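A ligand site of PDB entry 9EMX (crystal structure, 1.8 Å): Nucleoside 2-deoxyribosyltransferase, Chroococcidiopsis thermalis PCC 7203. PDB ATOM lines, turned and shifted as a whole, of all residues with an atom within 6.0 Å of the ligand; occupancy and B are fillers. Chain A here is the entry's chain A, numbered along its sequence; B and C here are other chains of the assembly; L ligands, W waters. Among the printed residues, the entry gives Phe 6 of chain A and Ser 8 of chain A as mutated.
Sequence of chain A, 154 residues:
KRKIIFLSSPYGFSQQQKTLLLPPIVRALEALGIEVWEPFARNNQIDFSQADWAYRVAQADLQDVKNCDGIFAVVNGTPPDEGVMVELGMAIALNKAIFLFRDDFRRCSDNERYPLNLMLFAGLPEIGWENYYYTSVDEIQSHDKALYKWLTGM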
ATOM      1  N   PHE A   6     -34.927 -32.339 -30.289  1.00  0.00           N
ATOM      2  CA  PHE A   6     -34.107 -31.310 -29.661  1.00  0.00           C
ATOM      3  C   PHE A   6     -34.679 -31.077 -28.264  1.00  0.00           C
ATOM      4  O   PHE A   6     -35.826 -30.629 -28.121  1.00  0.00           O
ATOM      5  CB  PHE A   6     -34.129 -30.037 -30.509  1.00  0.00           C
ATOM      6  CG  PHE A   6     -33.222 -28.942 -29.999  1.00  0.00           C
ATOM      7  CD1 PHE A   6     -31.879 -28.930 -30.309  1.00  0.00           C
ATOM      8  CD2 PHE A   6     -33.735 -27.909 -29.213  1.00  0.00           C
ATOM      9  CE1 PHE A   6     -31.061 -27.923 -29.851  1.00  0.00           C
ATOM     10  CE2 PHE A   6     -32.917 -26.889 -28.763  1.00  0.00           C
ATOM     11  CZ  PHE A   6     -31.578 -26.890 -29.079  1.00  0.00           C
ATOM     12  N   SER A   8     -34.832 -29.030 -25.328  1.00  0.00           N
ATOM     13  CA  SER A   8     -34.533 -27.657 -24.966  1.00  0.00           C
ATOM     14  C   SER A   8     -34.936 -27.444 -23.510  1.00  0.00           C
ATOM     15  O   SER A   8     -36.113 -27.586 -23.161  1.00  0.00           O
ATOM     16  CB  SER A   8     -35.285 -26.699 -25.898  1.00  0.00           C
ATOM     17  OG  SER A   8     -35.099 -25.365 -25.493  1.00  0.00           O
ATOM     18  N   SER A   9     -33.954 -27.136 -22.653  1.00  0.00           N
ATOM     19  CA  SER A   9     -34.210 -26.912 -21.235  1.00  0.00           C
ATOM     20  C   SER A   9     -33.279 -25.823 -20.725  1.00  0.00           C
ATOM     21  O   SER A   9     -32.282 -25.499 -21.355  1.00  0.00           O
ATOM     22  CB  SER A   9     -33.988 -28.170 -20.398  1.00  0.00           C
ATOM     23  OG  SER A   9     -32.591 -28.402 -20.217  1.00  0.00           O
ATOM     24  N   PRO A  10     -33.596 -25.240 -19.555  1.00  0.00           N
ATOM     25  CA  PRO A  10     -32.631 -24.371 -18.866  1.00  0.00           C
ATOM     26  C   PRO A  10     -31.750 -25.098 -17.868  1.00  0.00           C
ATOM     27  O   PRO A  10     -31.011 -24.453 -17.127  1.00  0.00           O
ATOM     28  CB  PRO A  10     -33.565 -23.398 -18.133  1.00  0.00           C
ATOM     29  CG  PRO A  10     -34.734 -24.275 -17.735  1.00  0.00           C
ATOM     30  CD  PRO A  10     -34.857 -25.355 -18.802  1.00  0.00           C
ATOM     31  N   PHE A  13     -27.844 -24.552 -16.968  1.00  0.00           N
ATOM     32  CA  PHE A  13     -27.318 -23.377 -16.289  1.00  0.00           C
ATOM     33  C   PHE A  13     -26.951 -23.635 -14.827  1.00  0.00           C
ATOM     34  O   PHE A  13     -26.246 -22.813 -14.227  1.00  0.00           O
ATOM     35  CB  PHE A  13     -28.331 -22.228 -16.356  1.00  0.00           C
ATOM     36  CG  PHE A  13     -28.499 -21.700 -17.737  1.00  0.00           C
ATOM     37  CD1 PHE A  13     -27.400 -21.272 -18.453  1.00  0.00           C
ATOM     38  CD2 PHE A  13     -29.754 -21.666 -18.323  1.00  0.00           C
ATOM     39  CE1 PHE A  13     -27.542 -20.790 -19.737  1.00  0.00           C
ATOM     40  CE2 PHE A  13     -29.911 -21.188 -19.610  1.00  0.00           C
ATOM     41  CZ  PHE A  13     -28.792 -20.750 -20.324  1.00  0.00           C
ATOM     42  N   PRO A  39     -28.787 -29.422 -26.214  1.00  0.00           N
ATOM     43  CA  PRO A  39     -27.797 -28.384 -26.589  1.00  0.00           C
ATOM     44  C   PRO A  39     -26.599 -28.240 -25.655  1.00  0.00           C
ATOM     45  O   PRO A  39     -25.526 -27.853 -26.124  1.00  0.00           O
ATOM     46  CB  PRO A  39     -28.640 -27.099 -26.616  1.00  0.00           C
ATOM     47  CG  PRO A  39     -29.856 -27.398 -25.799  1.00  0.00           C
ATOM     48  CD  PRO A  39     -30.132 -28.862 -25.989  1.00  0.00           C
ATOM     49  N   PHE A  40     -26.734 -28.475 -24.348  1.00  0.00           N
ATOM     50  CA  PHE A  40     -25.565 -28.287 -23.488  1.00  0.00           C
ATOM     51  C   PHE A  40     -24.521 -29.352 -23.787  1.00  0.00           C
ATOM     52  O   PHE A  40     -23.336 -29.025 -23.987  1.00  0.00           O
ATOM     53  CB  PHE A  40     -25.976 -28.277 -22.010  1.00  0.00           C
ATOM     54  CG  PHE A  40     -26.786 -27.045 -21.654  1.00  0.00           C
ATOM     55  CD1 PHE A  40     -26.164 -25.826 -21.428  1.00  0.00           C
ATOM     56  CD2 PHE A  40     -28.183 -27.090 -21.623  1.00  0.00           C
ATOM     57  CE1 PHE A  40     -26.898 -24.686 -21.161  1.00  0.00           C
ATOM     58  CE2 PHE A  40     -28.927 -25.940 -21.353  1.00  0.00           C
ATOM     59  CZ  PHE A  40     -28.292 -24.748 -21.130  1.00  0.00           C
ATOM     60  N   ASN A  43     -22.700 -28.971 -27.233  1.00  0.00           N
ATOM     61  CA  ASN A  43     -21.760 -27.866 -27.386  1.00  0.00           C
ATOM     62  C   ASN A  43     -20.588 -27.960 -26.417  1.00  0.00           C
ATOM     63  O   ASN A  43     -19.901 -26.946 -26.193  1.00  0.00           O
ATOM     64  CB  ASN A  43     -22.478 -26.522 -27.209  1.00  0.00           C
ATOM     65  CG  ASN A  43     -23.197 -26.066 -28.475  1.00  0.00           C
ATOM     66  OD1 ASN A  43     -22.593 -25.414 -29.329  1.00  0.00           O
ATOM     67  ND2 ASN A  43     -24.480 -26.370 -28.578  1.00  0.00           N
ATOM     68  N   PHE A  48     -14.638 -22.534 -24.651  1.00  0.00           N
ATOM     69  CA  PHE A  48     -15.309 -21.474 -23.913  1.00  0.00           C
ATOM     70  C   PHE A  48     -14.351 -20.409 -23.403  1.00  0.00           C
ATOM     71  O   PHE A  48     -14.793 -19.499 -22.690  1.00  0.00           O
ATOM     72  CB  PHE A  48     -16.124 -22.086 -22.756  1.00  0.00           C
ATOM     73  CG  PHE A  48     -17.203 -23.008 -23.223  1.00  0.00           C
ATOM     74  CD1 PHE A  48     -16.957 -24.353 -23.408  1.00  0.00           C
ATOM     75  CD2 PHE A  48     -18.472 -22.523 -23.546  1.00  0.00           C
ATOM     76  CE1 PHE A  48     -17.937 -25.212 -23.877  1.00  0.00           C
ATOM     77  CE2 PHE A  48     -19.465 -23.385 -24.019  1.00  0.00           C
ATOM     78  CZ  PHE A  48     -19.194 -24.731 -24.181  1.00  0.00           C
ATOM     79  N   TRP A  53     -17.400 -17.742 -28.251  1.00  0.00           N
ATOM     80  CA  TRP A  53     -18.101 -18.990 -27.977  1.00  0.00           C
ATOM     81  C   TRP A  53     -19.612 -18.795 -27.922  1.00  0.00           C
ATOM     82  O   TRP A  53     -20.368 -19.698 -28.298  1.00  0.00           O
ATOM     83  CB  TRP A  53     -17.616 -19.640 -26.679  1.00  0.00           C
ATOM     84  CG  TRP A  53     -18.049 -18.968 -25.407  1.00  0.00           C
ATOM     85  CD1 TRP A  53     -17.318 -18.083 -24.653  1.00  0.00           C
ATOM     86  CD2 TRP A  53     -19.290 -19.167 -24.696  1.00  0.00           C
ATOM     87  NE1 TRP A  53     -18.023 -17.718 -23.527  1.00  0.00           N
ATOM     88  CE2 TRP A  53     -19.235 -18.366 -23.535  1.00  0.00           C
ATOM     89  CE3 TRP A  53     -20.424 -19.946 -24.926  1.00  0.00           C
ATOM     90  CZ2 TRP A  53     -20.288 -18.314 -22.613  1.00  0.00           C
ATOM     91  CZ3 TRP A  53     -21.465 -19.885 -24.030  1.00  0.00           C
ATOM     92  CH2 TRP A  53     -21.395 -19.074 -22.882  1.00  0.00           C
ATOM     93  N   VAL A  57     -22.337 -21.062 -30.093  1.00  0.00           N
ATOM     94  CA  VAL A  57     -23.396 -21.844 -29.457  1.00  0.00           C
ATOM     95  C   VAL A  57     -24.765 -21.417 -30.000  1.00  0.00           C
ATOM     96  O   VAL A  57     -25.618 -22.271 -30.257  1.00  0.00           O
ATOM     97  CB  VAL A  57     -23.338 -21.694 -27.922  1.00  0.00           C
ATOM     98  CG1 VAL A  57     -24.645 -22.140 -27.281  1.00  0.00           C
ATOM     99  CG2 VAL A  57     -22.170 -22.498 -27.324  1.00  0.00           C
ATOM    100  N   ASP A  61     -27.227 -24.142 -31.807  1.00  0.00           N
ATOM    101  CA  ASP A  61     -28.610 -24.350 -31.407  1.00  0.00           C
ATOM    102  C   ASP A  61     -29.562 -23.993 -32.538  1.00  0.00           C
ATOM    103  O   ASP A  61     -30.528 -24.711 -32.807  1.00  0.00           O
ATOM    104  CB  ASP A  61     -28.943 -23.526 -30.154  1.00  0.00           C
ATOM    105  CG  ASP A  61     -28.215 -24.008 -28.906  1.00  0.00           C
ATOM    106  OD1 ASP A  61     -27.479 -25.017 -28.947  1.00  0.00           O
ATOM    107  OD2 ASP A  61     -28.372 -23.342 -27.862  1.00  0.00           O
ATOM    108  N   ASP A  81     -37.937 -20.452 -19.554  1.00  0.00           N
ATOM    109  CA  ASP A  81     -36.651 -19.894 -19.916  1.00  0.00           C
ATOM    110  C   ASP A  81     -36.697 -19.239 -21.293  1.00  0.00           C
ATOM    111  O   ASP A  81     -37.288 -19.772 -22.232  1.00  0.00           O
ATOM    112  CB  ASP A  81     -35.580 -20.992 -19.920  1.00  0.00           C
ATOM    113  CG  ASP A  81     -34.222 -20.469 -20.333  1.00  0.00           C
ATOM    114  OD1 ASP A  81     -33.504 -19.911 -19.486  1.00  0.00           O
ATOM    115  OD2 ASP A  81     -33.877 -20.597 -21.521  1.00  0.00           O
ATOM    116  N   GLU A  82     -36.026 -18.082 -21.414  1.00  0.00           N
ATOM    117  CA  GLU A  82     -36.119 -17.303 -22.638  1.00  0.00           C
ATOM    118  C   GLU A  82     -35.381 -17.961 -23.798  1.00  0.00           C
ATOM    119  O   GLU A  82     -35.798 -17.813 -24.945  1.00  0.00           O
ATOM    120  CB  GLU A  82     -35.609 -15.880 -22.366  1.00  0.00           C
ATOM    121  CG  GLU A  82     -34.145 -15.782 -21.967  1.00  0.00           C
ATOM    122  CD  GLU A  82     -33.882 -15.882 -20.454  1.00  0.00           C
ATOM    123  OE1 GLU A  82     -34.663 -16.503 -19.693  1.00  0.00           O
ATOM    124  OE2 GLU A  82     -32.858 -15.302 -20.022  1.00  0.00           O
ATOM    125  N   GLY A  83     -34.285 -18.694 -23.534  1.00  0.00           N
ATOM    126  CA  GLY A  83     -33.645 -19.467 -24.587  1.00  0.00           C
ATOM    127  C   GLY A  83     -34.538 -20.589 -25.101  1.00  0.00           C
ATOM    128  O   GLY A  83     -34.639 -20.824 -26.310  1.00  0.00           O
ATOM    129  N   VAL A  84     -35.182 -21.307 -24.174  1.00  0.00           N
ATOM    130  CA  VAL A  84     -36.143 -22.336 -24.571  1.00  0.00           C
ATOM    131  C   VAL A  84     -37.269 -21.701 -25.395  1.00  0.00           C
ATOM    132  O   VAL A  84     -37.742 -22.282 -26.384  1.00  0.00           O
ATOM    133  CB  VAL A  84     -36.696 -23.056 -23.332  1.00  0.00           C
ATOM    134  CG1 VAL A  84     -37.795 -24.045 -23.717  1.00  0.00           C
ATOM    135  CG2 VAL A  84     -35.557 -23.762 -22.571  1.00  0.00           C
ATOM    136  N   GLU A  87     -36.210 -20.976 -28.987  1.00  0.00           N
ATOM    137  CA  GLU A  87     -36.076 -22.223 -29.731  1.00  0.00           C
ATOM    138  C   GLU A  87     -37.436 -22.830 -30.034  1.00  0.00           C
ATOM    139  O   GLU A  87     -37.638 -23.400 -31.116  1.00  0.00           O
ATOM    140  CB  GLU A  87     -35.206 -23.203 -28.939  1.00  0.00           C
ATOM    141  CG  GLU A  87     -33.727 -22.779 -28.959  1.00  0.00           C
ATOM    142  CD  GLU A  87     -32.913 -23.263 -27.789  1.00  0.00           C
ATOM    143  OE1 GLU A  87     -33.450 -23.979 -26.910  1.00  0.00           O
ATOM    144  OE2 GLU A  87     -31.716 -22.904 -27.749  1.00  0.00           O
ATOM    145  N   ASP B 110     -25.106 -15.490 -19.187  1.00  0.00           N
ATOM    146  CA  ASP B 110     -24.009 -16.386 -18.839  1.00  0.00           C
ATOM    147  C   ASP B 110     -22.776 -16.176 -19.718  1.00  0.00           C
ATOM    148  O   ASP B 110     -21.899 -17.048 -19.754  1.00  0.00           O
ATOM    149  CB  ASP B 110     -24.462 -17.828 -18.958  1.00  0.00           C
ATOM    150  CG  ASP B 110     -24.639 -18.245 -20.414  1.00  0.00           C
ATOM    151  OD1 ASP B 110     -24.769 -17.338 -21.265  1.00  0.00           O
ATOM    152  OD2 ASP B 110     -24.639 -19.473 -20.694  1.00  0.00           O
ATOM    153  N   ASN B 117     -29.387 -13.701 -22.564  1.00  0.00           N
ATOM    154  CA  ASN B 117     -29.223 -15.059 -23.085  1.00  0.00           C
ATOM    155  C   ASN B 117     -28.807 -15.003 -24.551  1.00  0.00           C
ATOM    156  O   ASN B 117     -29.388 -14.245 -25.340  1.00  0.00           O
ATOM    157  CB  ASN B 117     -30.526 -15.843 -22.899  1.00  0.00           C
ATOM    158  CG  ASN B 117     -30.441 -17.285 -23.387  1.00  0.00           C
ATOM    159  OD1 ASN B 117     -30.108 -17.529 -24.547  1.00  0.00           O
ATOM    160  ND2 ASN B 117     -30.729 -18.243 -22.508  1.00  0.00           N
ATOM    161  N   LEU B 118     -27.773 -15.796 -24.919  1.00  0.00           N
ATOM    162  CA  LEU B 118     -27.183 -15.691 -26.255  1.00  0.00           C
ATOM    163  C   LEU B 118     -28.172 -15.987 -27.377  1.00  0.00           C
ATOM    164  O   LEU B 118     -27.987 -15.513 -28.504  1.00  0.00           O
ATOM    165  CB  LEU B 118     -25.964 -16.602 -26.389  1.00  0.00           C
ATOM    166  CG  LEU B 118     -26.104 -18.098 -26.050  1.00  0.00           C
ATOM    167  CD1 LEU B 118     -26.575 -18.915 -27.287  1.00  0.00           C
ATOM    168  CD2 LEU B 118     -24.801 -18.679 -25.439  1.00  0.00           C
ATOM    169  N   MET B 119     -29.206 -16.793 -27.119  1.00  0.00           N
ATOM    170  CA  MET B 119     -30.136 -17.102 -28.200  1.00  0.00           C
ATOM    171  C   MET B 119     -30.927 -15.884 -28.680  1.00  0.00           C
ATOM    172  O   MET B 119     -31.394 -15.882 -29.830  1.00  0.00           O
ATOM    173  CB  MET B 119     -31.099 -18.209 -27.751  1.00  0.00           C
ATOM    174  CG  MET B 119     -30.416 -19.547 -27.591  1.00  0.00           C
ATOM    175  SD  MET B 119     -29.669 -20.149 -29.132  1.00  0.00           S
ATOM    176  CE  MET B 119     -31.002 -19.937 -30.312  1.00  0.00           C
ATOM    177  N   PHE C 105     -24.820 -20.560 -13.309  1.00  0.00           N
ATOM    178  CA  PHE C 105     -23.685 -19.727 -13.681  1.00  0.00           C
ATOM    179  C   PHE C 105     -24.089 -18.481 -14.453  1.00  0.00           C
ATOM    180  O   PHE C 105     -23.206 -17.735 -14.899  1.00  0.00           O
ATOM    181  CB  PHE C 105     -22.629 -20.555 -14.433  1.00  0.00           C
ATOM    182  CG  PHE C 105     -23.021 -20.993 -15.806  1.00  0.00           C
ATOM    183  CD1 PHE C 105     -22.989 -20.087 -16.879  1.00  0.00           C
ATOM    184  CD2 PHE C 105     -23.335 -22.326 -16.075  1.00  0.00           C
ATOM    185  CE1 PHE C 105     -23.317 -20.497 -18.198  1.00  0.00           C
ATOM    186  CE2 PHE C 105     -23.659 -22.735 -17.381  1.00  0.00           C
ATOM    187  CZ  PHE C 105     -23.658 -21.818 -18.459  1.00  0.00           C
HETATM  188  O1  LIG L   1     -31.545 -20.882 -22.483  1.00  0.00           O
HETATM  189  C1  LIG L   1     -31.336 -22.242 -22.782  1.00  0.00           C
HETATM  190  C2  LIG L   1     -31.723 -22.547 -24.196  1.00  0.00           C
HETATM  191  O2  LIG L   1     -30.989 -21.737 -25.146  1.00  0.00           O
HETATM  192  C3  LIG L   1     -31.309 -23.976 -24.454  1.00  0.00           C
HETATM  193  C4  LIG L   1     -29.983 -23.793 -25.199  1.00  0.00           C
HETATM  194  O3  LIG L   1     -30.009 -24.538 -26.407  1.00  0.00           O
HETATM  195  C5  LIG L   1     -29.796 -22.298 -25.546  1.00  0.00           C
HETATM  196  N1  LIG L   1     -28.605 -21.809 -24.794  1.00  0.00           N
HETATM  197  C6  LIG L   1     -28.486 -20.615 -24.136  1.00  0.00           C
HETATM  198  N2  LIG L   1     -27.344 -20.467 -23.541  1.00  0.00           N
HETATM  199  C7  LIG L   1     -26.663 -21.630 -23.813  1.00  0.00           C
HETATM  200  C8  LIG L   1     -25.393 -22.081 -23.461  1.00  0.00           C
HETATM  201  N3  LIG L   1     -24.566 -21.334 -22.712  1.00  0.00           N
HETATM  202  N4  LIG L   1     -25.000 -23.287 -23.895  1.00  0.00           N
HETATM  203  C9  LIG L   1     -25.824 -24.022 -24.638  1.00  0.00           C
HETATM  204  N5  LIG L   1     -27.031 -23.696 -25.051  1.00  0.00           N
HETATM  205  C10 LIG L   1     -27.417 -22.478 -24.598  1.00  0.00           C
HETATM  206  O   HOH W   1     -26.830 -17.704 -22.591  1.00  0.00           O
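The side-chain carboxylate of Asp 61 lies within hydrogen-bond range of an oxygen (O3) of the ligand.
O1 of the ligand sits at hydrogen-bond distance from OD2 of Asp 81.
OE2 of Glu 87 sits at hydrogen-bond distance from O3 of the ligand, 2.7 Å away.
OD2 of Asp 110 of chain B is in hydrogen-bond range of N3 of the ligand (2.7 Å).
The side-chain amide nitrogen (ND2) of Asn 117 of chain B lies within hydrogen-bond range of an oxygen (O1) of the ligand (2.8 Å).
OD1 of Asp 61 lies within hydrogen-bond range of ND2 of Asn 43, at 3.3 Å.
The side-chain carboxylate (OD2) of Asp 81 sits at hydrogen-bond distance from the backbone NH (N) of Gly 83 (2.8 Å).
The side-chain carboxylate of Asp 81 sits at hydrogen-bond distance from the backbone NH of Val 84 (3.0 Å).
OG of Ser 8 is in hydrogen-bond range of OE1 of Glu 87, 2.6 Å away.
The side-chain amide oxygen (OD1) of Asn 117 of chain B is in hydrogen-bond range of the backbone NH (N) of Met 119 of chain B, at 2.8 Å.
The backbone carbonyl oxygen (O) of Pro 39 lies within hydrogen-bond range of the side-chain amide nitrogen (ND2) of Asn 43 (3.1 Å).
The backbone NH (N) of Phe 105 of chain C sits at hydrogen-bond distance from the backbone carbonyl oxygen (O) of Phe 13, 2.8 Å away.
Water W1 lies within hydrogen-bond range of the side-chain carboxylate (OD1) of Asp 110 of chain B, a nitrogen (N2) of the ligand and the backbone NH (N) of Leu 118 of chain B.
Phe 6 touches the ligand.
O of Ser 9 touches C3 of the ligand, 3.6 Å away.
Phe 13 touches the ligand.
CB of Pro 39 touches O3 of the ligand, 2.9 Å away.
Phe 40 touches the ligand (CE1 to N4, 3.6 Å).
Trp 53 touches the ligand (CZ3 to N3, 3.7 Å).
CG1 of Val 57 touches C9 of the ligand, 3.5 Å away.
Gly 83 touches the ligand.
Val 84 touches the ligand.
Leu 118 of chain B touches the ligand (CD2 to N2, 3.6 Å).
Met 119 of chain B touches the ligand (CG to O2, 3.3 Å).
Hydrophobic or aromatic side chains within 4 Å of the ligand: Phe 6, Phe 13, Pro 39, Phe 40, Trp 53, Val 57, Leu 118 of chain B and Met 119 of chain B.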
